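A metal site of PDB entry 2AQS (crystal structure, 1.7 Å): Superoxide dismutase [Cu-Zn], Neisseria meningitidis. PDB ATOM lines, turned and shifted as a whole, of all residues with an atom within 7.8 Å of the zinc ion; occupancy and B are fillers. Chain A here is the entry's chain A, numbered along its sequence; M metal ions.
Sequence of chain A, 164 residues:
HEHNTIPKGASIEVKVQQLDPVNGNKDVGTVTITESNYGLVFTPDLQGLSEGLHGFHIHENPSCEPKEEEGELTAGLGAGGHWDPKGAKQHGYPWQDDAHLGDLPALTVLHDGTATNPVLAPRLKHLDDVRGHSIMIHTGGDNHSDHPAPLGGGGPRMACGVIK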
ATOM      1  N   PHE A  56      32.178  -6.457  30.570  1.00  0.00           N
ATOM      2  CA  PHE A  56      32.171  -6.682  32.004  1.00  0.00           C
ATOM      3  C   PHE A  56      31.173  -7.803  32.287  1.00  0.00           C
ATOM      4  O   PHE A  56      29.986  -7.638  32.072  1.00  0.00           O
ATOM      5  CB  PHE A  56      31.751  -5.349  32.645  1.00  0.00           C
ATOM      6  CG  PHE A  56      31.832  -5.314  34.140  1.00  0.00           C
ATOM      7  CD1 PHE A  56      32.957  -5.789  34.802  1.00  0.00           C
ATOM      8  CD2 PHE A  56      30.819  -4.705  34.876  1.00  0.00           C
ATOM      9  CE1 PHE A  56      33.067  -5.660  36.175  1.00  0.00           C
ATOM     10  CE2 PHE A  56      30.918  -4.564  36.247  1.00  0.00           C
ATOM     11  CZ  PHE A  56      32.039  -5.036  36.900  1.00  0.00           C
ATOM     12  N   HIS A  57      31.670  -8.962  32.731  1.00  0.00           N
ATOM     13  CA  HIS A  57      30.792 -10.096  33.013  1.00  0.00           C
ATOM     14  C   HIS A  57      31.204 -10.955  34.196  1.00  0.00           C
ATOM     15  O   HIS A  57      32.369 -10.971  34.613  1.00  0.00           O
ATOM     16  CB  HIS A  57      30.696 -11.055  31.817  1.00  0.00           C
ATOM     17  CG  HIS A  57      30.993 -10.420  30.489  1.00  0.00           C
ATOM     18  ND1 HIS A  57      32.177 -10.628  29.819  1.00  0.00           N
ATOM     19  CD2 HIS A  57      30.236  -9.625  29.690  1.00  0.00           C
ATOM     20  CE1 HIS A  57      32.152  -9.978  28.673  1.00  0.00           C
ATOM     21  NE2 HIS A  57      30.981  -9.359  28.562  1.00  0.00           N
ATOM     22  N   ILE A  58      30.237 -11.679  34.742  1.00  0.00           N
ATOM     23  CA  ILE A  58      30.496 -12.602  35.827  1.00  0.00           C
ATOM     24  C   ILE A  58      30.839 -13.915  35.114  1.00  0.00           C
ATOM     25  O   ILE A  58      30.120 -14.343  34.206  1.00  0.00           O
ATOM     26  CB  ILE A  58      29.236 -12.829  36.709  1.00  0.00           C
ATOM     27  CG1 ILE A  58      28.789 -11.494  37.316  1.00  0.00           C
ATOM     28  CG2 ILE A  58      29.525 -13.877  37.766  1.00  0.00           C
ATOM     29  CD1 ILE A  58      29.753 -10.865  38.276  1.00  0.00           C
ATOM     30  N   HIS A  59      31.941 -14.537  35.503  1.00  0.00           N
ATOM     31  CA  HIS A  59      32.344 -15.793  34.904  1.00  0.00           C
ATOM     32  C   HIS A  59      32.094 -16.918  35.896  1.00  0.00           C
ATOM     33  O   HIS A  59      32.057 -16.695  37.102  1.00  0.00           O
ATOM     34  CB  HIS A  59      33.807 -15.735  34.438  1.00  0.00           C
ATOM     35  CG  HIS A  59      33.989 -14.991  33.148  1.00  0.00           C
ATOM     36  ND1 HIS A  59      34.529 -15.570  32.020  1.00  0.00           N
ATOM     37  CD2 HIS A  59      33.653 -13.726  32.789  1.00  0.00           C
ATOM     38  CE1 HIS A  59      34.520 -14.694  31.025  1.00  0.00           C
ATOM     39  NE2 HIS A  59      33.987 -13.569  31.472  1.00  0.00           N
ATOM     40  N   GLY A  81      33.929 -19.813  31.378  1.00  0.00           N
ATOM     41  CA  GLY A  81      33.149 -18.954  30.496  1.00  0.00           C
ATOM     42  C   GLY A  81      32.191 -18.024  31.234  1.00  0.00           C
ATOM     43  O   GLY A  81      32.231 -17.914  32.463  1.00  0.00           O
ATOM     44  N   HIS A  82      31.345 -17.324  30.481  1.00  0.00           N
ATOM     45  CA  HIS A  82      30.381 -16.430  31.098  1.00  0.00           C
ATOM     46  C   HIS A  82      29.456 -17.244  31.984  1.00  0.00           C
ATOM     47  O   HIS A  82      29.007 -18.322  31.592  1.00  0.00           O
ATOM     48  CB  HIS A  82      29.543 -15.708  30.030  1.00  0.00           C
ATOM     49  CG  HIS A  82      30.313 -14.713  29.221  1.00  0.00           C
ATOM     50  ND1 HIS A  82      29.694 -13.747  28.469  1.00  0.00           N
ATOM     51  CD2 HIS A  82      31.644 -14.543  29.040  1.00  0.00           C
ATOM     52  CE1 HIS A  82      30.604 -13.017  27.848  1.00  0.00           C
ATOM     53  NE2 HIS A  82      31.803 -13.478  28.174  1.00  0.00           N
ATOM     54  N   TRP A  83      29.184 -16.732  33.177  1.00  0.00           N
ATOM     55  CA  TRP A  83      28.293 -17.417  34.109  1.00  0.00           C
ATOM     56  C   TRP A  83      26.898 -17.494  33.461  1.00  0.00           C
ATOM     57  O   TRP A  83      26.274 -16.480  33.179  1.00  0.00           O
ATOM     58  CB  TRP A  83      28.225 -16.636  35.416  1.00  0.00           C
ATOM     59  CG  TRP A  83      27.466 -17.334  36.489  1.00  0.00           C
ATOM     60  CD1 TRP A  83      27.545 -18.650  36.834  1.00  0.00           C
ATOM     61  CD2 TRP A  83      26.535 -16.737  37.400  1.00  0.00           C
ATOM     62  NE1 TRP A  83      26.729 -18.910  37.905  1.00  0.00           N
ATOM     63  CE2 TRP A  83      26.093 -17.757  38.270  1.00  0.00           C
ATOM     64  CE3 TRP A  83      26.041 -15.435  37.565  1.00  0.00           C
ATOM     65  CZ2 TRP A  83      25.171 -17.519  39.298  1.00  0.00           C
ATOM     66  CZ3 TRP A  83      25.119 -15.197  38.593  1.00  0.00           C
ATOM     67  CH2 TRP A  83      24.696 -16.237  39.437  1.00  0.00           C
ATOM     68  N   ASP A  84      26.443 -18.734  33.250  1.00  0.00           N
ATOM     69  CA  ASP A  84      25.159 -18.987  32.591  1.00  0.00           C
ATOM     70  C   ASP A  84      24.402 -20.107  33.288  1.00  0.00           C
ATOM     71  O   ASP A  84      24.117 -21.155  32.695  1.00  0.00           O
ATOM     72  CB  ASP A  84      25.462 -19.334  31.127  1.00  0.00           C
ATOM     73  CG  ASP A  84      24.224 -19.551  30.299  1.00  0.00           C
ATOM     74  OD1 ASP A  84      23.224 -18.861  30.531  1.00  0.00           O
ATOM     75  OD2 ASP A  84      24.274 -20.401  29.388  1.00  0.00           O
ATOM     76  N   GLN A  90      23.719 -18.105  25.201  1.00  0.00           N
ATOM     77  CA  GLN A  90      23.991 -17.027  24.265  1.00  0.00           C
ATOM     78  C   GLN A  90      24.272 -15.734  25.034  1.00  0.00           C
ATOM     79  O   GLN A  90      23.703 -15.512  26.103  1.00  0.00           O
ATOM     80  CB  GLN A  90      22.832 -16.811  23.281  1.00  0.00           C
ATOM     81  CG  GLN A  90      21.508 -16.418  23.898  1.00  0.00           C
ATOM     82  CD  GLN A  90      20.462 -16.074  22.845  1.00  0.00           C
ATOM     83  OE1 GLN A  90      20.717 -16.166  21.648  1.00  0.00           O
ATOM     84  NE2 GLN A  90      19.278 -15.673  23.288  1.00  0.00           N
ATOM     85  N   HIS A  91      25.156 -14.908  24.476  1.00  0.00           N
ATOM     86  CA  HIS A  91      25.534 -13.642  25.081  1.00  0.00           C
ATOM     87  C   HIS A  91      24.544 -12.553  24.690  1.00  0.00           C
ATOM     88  O   HIS A  91      24.110 -12.485  23.530  1.00  0.00           O
ATOM     89  CB  HIS A  91      26.946 -13.248  24.647  1.00  0.00           C
ATOM     90  CG  HIS A  91      27.437 -11.989  25.279  1.00  0.00           C
ATOM     91  ND1 HIS A  91      27.760 -11.917  26.620  1.00  0.00           N
ATOM     92  CD2 HIS A  91      27.630 -10.757  24.776  1.00  0.00           C
ATOM     93  CE1 HIS A  91      28.132 -10.678  26.912  1.00  0.00           C
ATOM     94  NE2 HIS A  91      28.066  -9.955  25.806  1.00  0.00           N
ATOM     95  N   GLY A  92      24.177 -11.711  25.637  1.00  0.00           N
ATOM     96  CA  GLY A  92      23.207 -10.673  25.324  1.00  0.00           C
ATOM     97  C   GLY A  92      23.271  -9.456  26.213  1.00  0.00           C
ATOM     98  O   GLY A  92      24.327  -9.138  26.777  1.00  0.00           O
ATOM     99  N   TYR A  93      22.141  -8.759  26.335  1.00  0.00           N
ATOM    100  CA  TYR A  93      22.027  -7.554  27.153  1.00  0.00           C
ATOM    101  C   TYR A  93      21.805  -7.848  28.617  1.00  0.00           C
ATOM    102  O   TYR A  93      21.337  -8.934  28.980  1.00  0.00           O
ATOM    103  CB  TYR A  93      20.851  -6.709  26.658  1.00  0.00           C
ATOM    104  CG  TYR A  93      21.021  -6.171  25.267  1.00  0.00           C
ATOM    105  CD1 TYR A  93      21.825  -5.061  25.022  1.00  0.00           C
ATOM    106  CD2 TYR A  93      20.387  -6.775  24.178  1.00  0.00           C
ATOM    107  CE1 TYR A  93      21.986  -4.554  23.739  1.00  0.00           C
ATOM    108  CE2 TYR A  93      20.550  -6.286  22.878  1.00  0.00           C
ATOM    109  CZ  TYR A  93      21.350  -5.173  22.670  1.00  0.00           C
ATOM    110  OH  TYR A  93      21.533  -4.675  21.409  1.00  0.00           O
ATOM    111  N   ALA A  99      19.729 -14.360  27.983  1.00  0.00           N
ATOM    112  CA  ALA A  99      21.151 -14.078  27.829  1.00  0.00           C
ATOM    113  C   ALA A  99      21.853 -14.577  29.103  1.00  0.00           C
ATOM    114  O   ALA A  99      21.212 -14.758  30.130  1.00  0.00           O
ATOM    115  CB  ALA A  99      21.358 -12.577  27.672  1.00  0.00           C
ATOM    116  N   HIS A 100      23.166 -14.790  29.032  1.00  0.00           N
ATOM    117  CA  HIS A 100      23.898 -15.262  30.199  1.00  0.00           C
ATOM    118  C   HIS A 100      23.537 -14.399  31.389  1.00  0.00           C
ATOM    119  O   HIS A 100      23.510 -13.171  31.266  1.00  0.00           O
ATOM    120  CB  HIS A 100      25.407 -15.140  29.981  1.00  0.00           C
ATOM    121  CG  HIS A 100      25.926 -15.831  28.761  1.00  0.00           C
ATOM    122  ND1 HIS A 100      26.868 -15.273  27.938  1.00  0.00           N
ATOM    123  CD2 HIS A 100      25.663 -17.057  28.252  1.00  0.00           C
ATOM    124  CE1 HIS A 100      27.166 -16.117  26.964  1.00  0.00           C
ATOM    125  NE2 HIS A 100      26.447 -17.216  27.129  1.00  0.00           N
ATOM    126  N   LEU A 101      23.268 -15.013  32.540  1.00  0.00           N
ATOM    127  CA  LEU A 101      22.935 -14.240  33.736  1.00  0.00           C
ATOM    128  C   LEU A 101      24.120 -13.375  34.156  1.00  0.00           C
ATOM    129  O   LEU A 101      23.961 -12.376  34.853  1.00  0.00           O
ATOM    130  CB  LEU A 101      22.538 -15.179  34.871  1.00  0.00           C
ATOM    131  CG  LEU A 101      22.015 -14.485  36.128  1.00  0.00           C
ATOM    132  CD1 LEU A 101      20.797 -13.640  35.777  1.00  0.00           C
ATOM    133  CD2 LEU A 101      21.680 -15.506  37.200  1.00  0.00           C
ATOM    134  N   GLY A 102      25.319 -13.749  33.714  1.00  0.00           N
ATOM    135  CA  GLY A 102      26.509 -12.998  34.074  1.00  0.00           C
ATOM    136  C   GLY A 102      26.809 -11.802  33.195  1.00  0.00           C
ATOM    137  O   GLY A 102      27.821 -11.131  33.408  1.00  0.00           O
ATOM    138  N   ASP A 103      25.936 -11.501  32.234  1.00  0.00           N
ATOM    139  CA  ASP A 103      26.162 -10.379  31.331  1.00  0.00           C
ATOM    140  C   ASP A 103      25.818  -9.051  31.971  1.00  0.00           C
ATOM    141  O   ASP A 103      24.644  -8.709  32.143  1.00  0.00           O
ATOM    142  CB  ASP A 103      25.371 -10.577  30.037  1.00  0.00           C
ATOM    143  CG  ASP A 103      25.875 -11.770  29.242  1.00  0.00           C
ATOM    144  OD1 ASP A 103      26.991 -12.239  29.534  1.00  0.00           O
ATOM    145  OD2 ASP A 103      25.158 -12.237  28.322  1.00  0.00           O
ATOM    146  N   LEU A 104      26.842  -8.288  32.330  1.00  0.00           N
ATOM    147  CA  LEU A 104      26.656  -6.992  32.980  1.00  0.00           C
ATOM    148  C   LEU A 104      26.814  -5.829  31.996  1.00  0.00           C
ATOM    149  O   LEU A 104      27.243  -6.030  30.859  1.00  0.00           O
ATOM    150  CB  LEU A 104      27.680  -6.828  34.115  1.00  0.00           C
ATOM    151  CG  LEU A 104      27.913  -8.002  35.080  1.00  0.00           C
ATOM    152  CD1 LEU A 104      29.040  -7.646  36.044  1.00  0.00           C
ATOM    153  CD2 LEU A 104      26.640  -8.347  35.842  1.00  0.00           C
ATOM    154  N   ARG A 123      18.898  -8.281  36.380  1.00  0.00           N
ATOM    155  CA  ARG A 123      18.520  -9.684  36.530  1.00  0.00           C
ATOM    156  C   ARG A 123      19.134 -10.373  37.753  1.00  0.00           C
ATOM    157  O   ARG A 123      18.748 -11.484  38.105  1.00  0.00           O
ATOM    158  CB  ARG A 123      18.846 -10.449  35.248  1.00  0.00           C
ATOM    159  CG  ARG A 123      17.943 -10.059  34.088  1.00  0.00           C
ATOM    160  CD  ARG A 123      18.218 -10.922  32.880  1.00  0.00           C
ATOM    161  NE  ARG A 123      19.506 -10.630  32.256  1.00  0.00           N
ATOM    162  CZ  ARG A 123      20.363 -11.545  31.839  1.00  0.00           C
ATOM    163  NH1 ARG A 123      20.096 -12.845  31.991  1.00  0.00           N
ATOM    164  NH2 ARG A 123      21.484 -11.174  31.244  1.00  0.00           N
ATOM    165  N   ASP A 142      31.637  -4.493  24.473  1.00  0.00           N
ATOM    166  CA  ASP A 142      30.546  -5.449  24.551  1.00  0.00           C
ATOM    167  C   ASP A 142      29.326  -4.908  23.816  1.00  0.00           C
ATOM    168  O   ASP A 142      28.702  -3.943  24.268  1.00  0.00           O
ATOM    169  CB  ASP A 142      30.194  -5.689  26.033  1.00  0.00           C
ATOM    170  CG  ASP A 142      29.291  -6.905  26.234  1.00  0.00           C
ATOM    171  OD1 ASP A 142      28.660  -7.357  25.258  1.00  0.00           O
ATOM    172  OD2 ASP A 142      29.213  -7.390  27.384  1.00  0.00           O
ATOM    173  N   HIS A 144      26.787  -6.731  23.341  1.00  0.00           N
ATOM    174  CA  HIS A 144      25.725  -7.586  23.857  1.00  0.00           C
ATOM    175  C   HIS A 144      25.096  -8.531  22.847  1.00  0.00           C
ATOM    176  O   HIS A 144      23.874  -8.693  22.788  1.00  0.00           O
ATOM    177  CB  HIS A 144      24.660  -6.714  24.523  1.00  0.00           C
ATOM    178  CG  HIS A 144      25.198  -5.879  25.644  1.00  0.00           C
ATOM    179  ND1 HIS A 144      25.641  -6.422  26.828  1.00  0.00           N
ATOM    180  CD2 HIS A 144      25.391  -4.545  25.750  1.00  0.00           C
ATOM    181  CE1 HIS A 144      26.079  -5.467  27.620  1.00  0.00           C
ATOM    182  NE2 HIS A 144      25.939  -4.309  26.994  1.00  0.00           N
ATOM    183  N   SER A 145      25.955  -9.159  22.049  1.00  0.00           N
ATOM    184  CA  SER A 145      25.514 -10.098  21.036  1.00  0.00           C
ATOM    185  C   SER A 145      26.678 -11.024  20.729  1.00  0.00           C
ATOM    186  O   SER A 145      27.819 -10.708  21.028  1.00  0.00           O
ATOM    187  CB  SER A 145      25.107  -9.357  19.770  1.00  0.00           C
ATOM    188  OG  SER A 145      24.718 -10.263  18.744  1.00  0.00           O
ATOM    189  N   ASP A 146      26.365 -12.166  20.121  1.00  0.00           N
ATOM    190  CA  ASP A 146      27.393 -13.118  19.719  1.00  0.00           C
ATOM    191  C   ASP A 146      27.742 -12.870  18.253  1.00  0.00           C
ATOM    192  O   ASP A 146      28.468 -13.653  17.627  1.00  0.00           O
ATOM    193  CB  ASP A 146      26.911 -14.558  19.892  1.00  0.00           C
ATOM    194  CG  ASP A 146      26.994 -15.020  21.330  1.00  0.00           C
ATOM    195  OD1 ASP A 146      28.092 -14.944  21.917  1.00  0.00           O
ATOM    196  OD2 ASP A 146      25.954 -15.465  21.854  1.00  0.00           O
ATOM    197  N   LEU A 151      30.591 -13.498  22.195  1.00  0.00           N
ATOM    198  CA  LEU A 151      30.639 -12.864  23.497  1.00  0.00           C
ATOM    199  C   LEU A 151      30.790 -11.333  23.499  1.00  0.00           C
ATOM    200  O   LEU A 151      31.540 -10.776  24.305  1.00  0.00           O
ATOM    201  CB  LEU A 151      31.768 -13.509  24.322  1.00  0.00           C
ATOM    202  CG  LEU A 151      31.657 -15.045  24.357  1.00  0.00           C
ATOM    203  CD1 LEU A 151      32.940 -15.665  24.916  1.00  0.00           C
ATOM    204  CD2 LEU A 151      30.450 -15.440  25.199  1.00  0.00           C
ATOM    205  N   GLY A 152      30.071 -10.670  22.599  1.00  0.00           N
ATOM    206  CA  GLY A 152      30.093  -9.219  22.555  1.00  0.00           C
ATOM    207  C   GLY A 152      31.362  -8.530  22.090  1.00  0.00           C
ATOM    208  O   GLY A 152      31.467  -7.298  22.172  1.00  0.00           O
HETATM  209 ZN    ZN M   1      27.705 -13.400  28.144  1.00  0.00          ZN
HETATM  210 CU    CU M   2      33.667 -11.950  30.349  1.00  0.00          CU
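Of the 25 residues printed, 4 come within 4 Å of the zinc ion.
A ring nitrogen (ND1) of His 57 lies close to a ring nitrogen (NE2) of His 82, 3.3 Å away.
A ring nitrogen (NE2) of His 91 is in hydrogen-bond range of the side-chain carboxylate (OD1) of Asp 142 (2.7 Å).
The backbone NH (N) of His 91 is in hydrogen-bond range of the side-chain carboxylate (OD2) of Asp 146 (2.8 Å).
NH2 of Arg 123 is in hydrogen-bond range of O of His 100 (2.8 Å).
N of His 100 lies within hydrogen-bond range of O of Gln 90, 3.1 Å away.
The side-chain carboxylate (OD2) of Asp 103 lies within hydrogen-bond range of the backbone NH (N) of Gly 92, at 2.9 Å.
The zinc ion is bound by the side-chain carboxylate (OD1) of Asp 103, a ring nitrogen (ND1) of His 82, a ring nitrogen (ND1) of His 100 and a ring nitrogen (ND1) of His 91.
Slightly farther from the zinc ion lies the side-chain carboxylate (OD2) of Asp 103 (2.8 Å).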
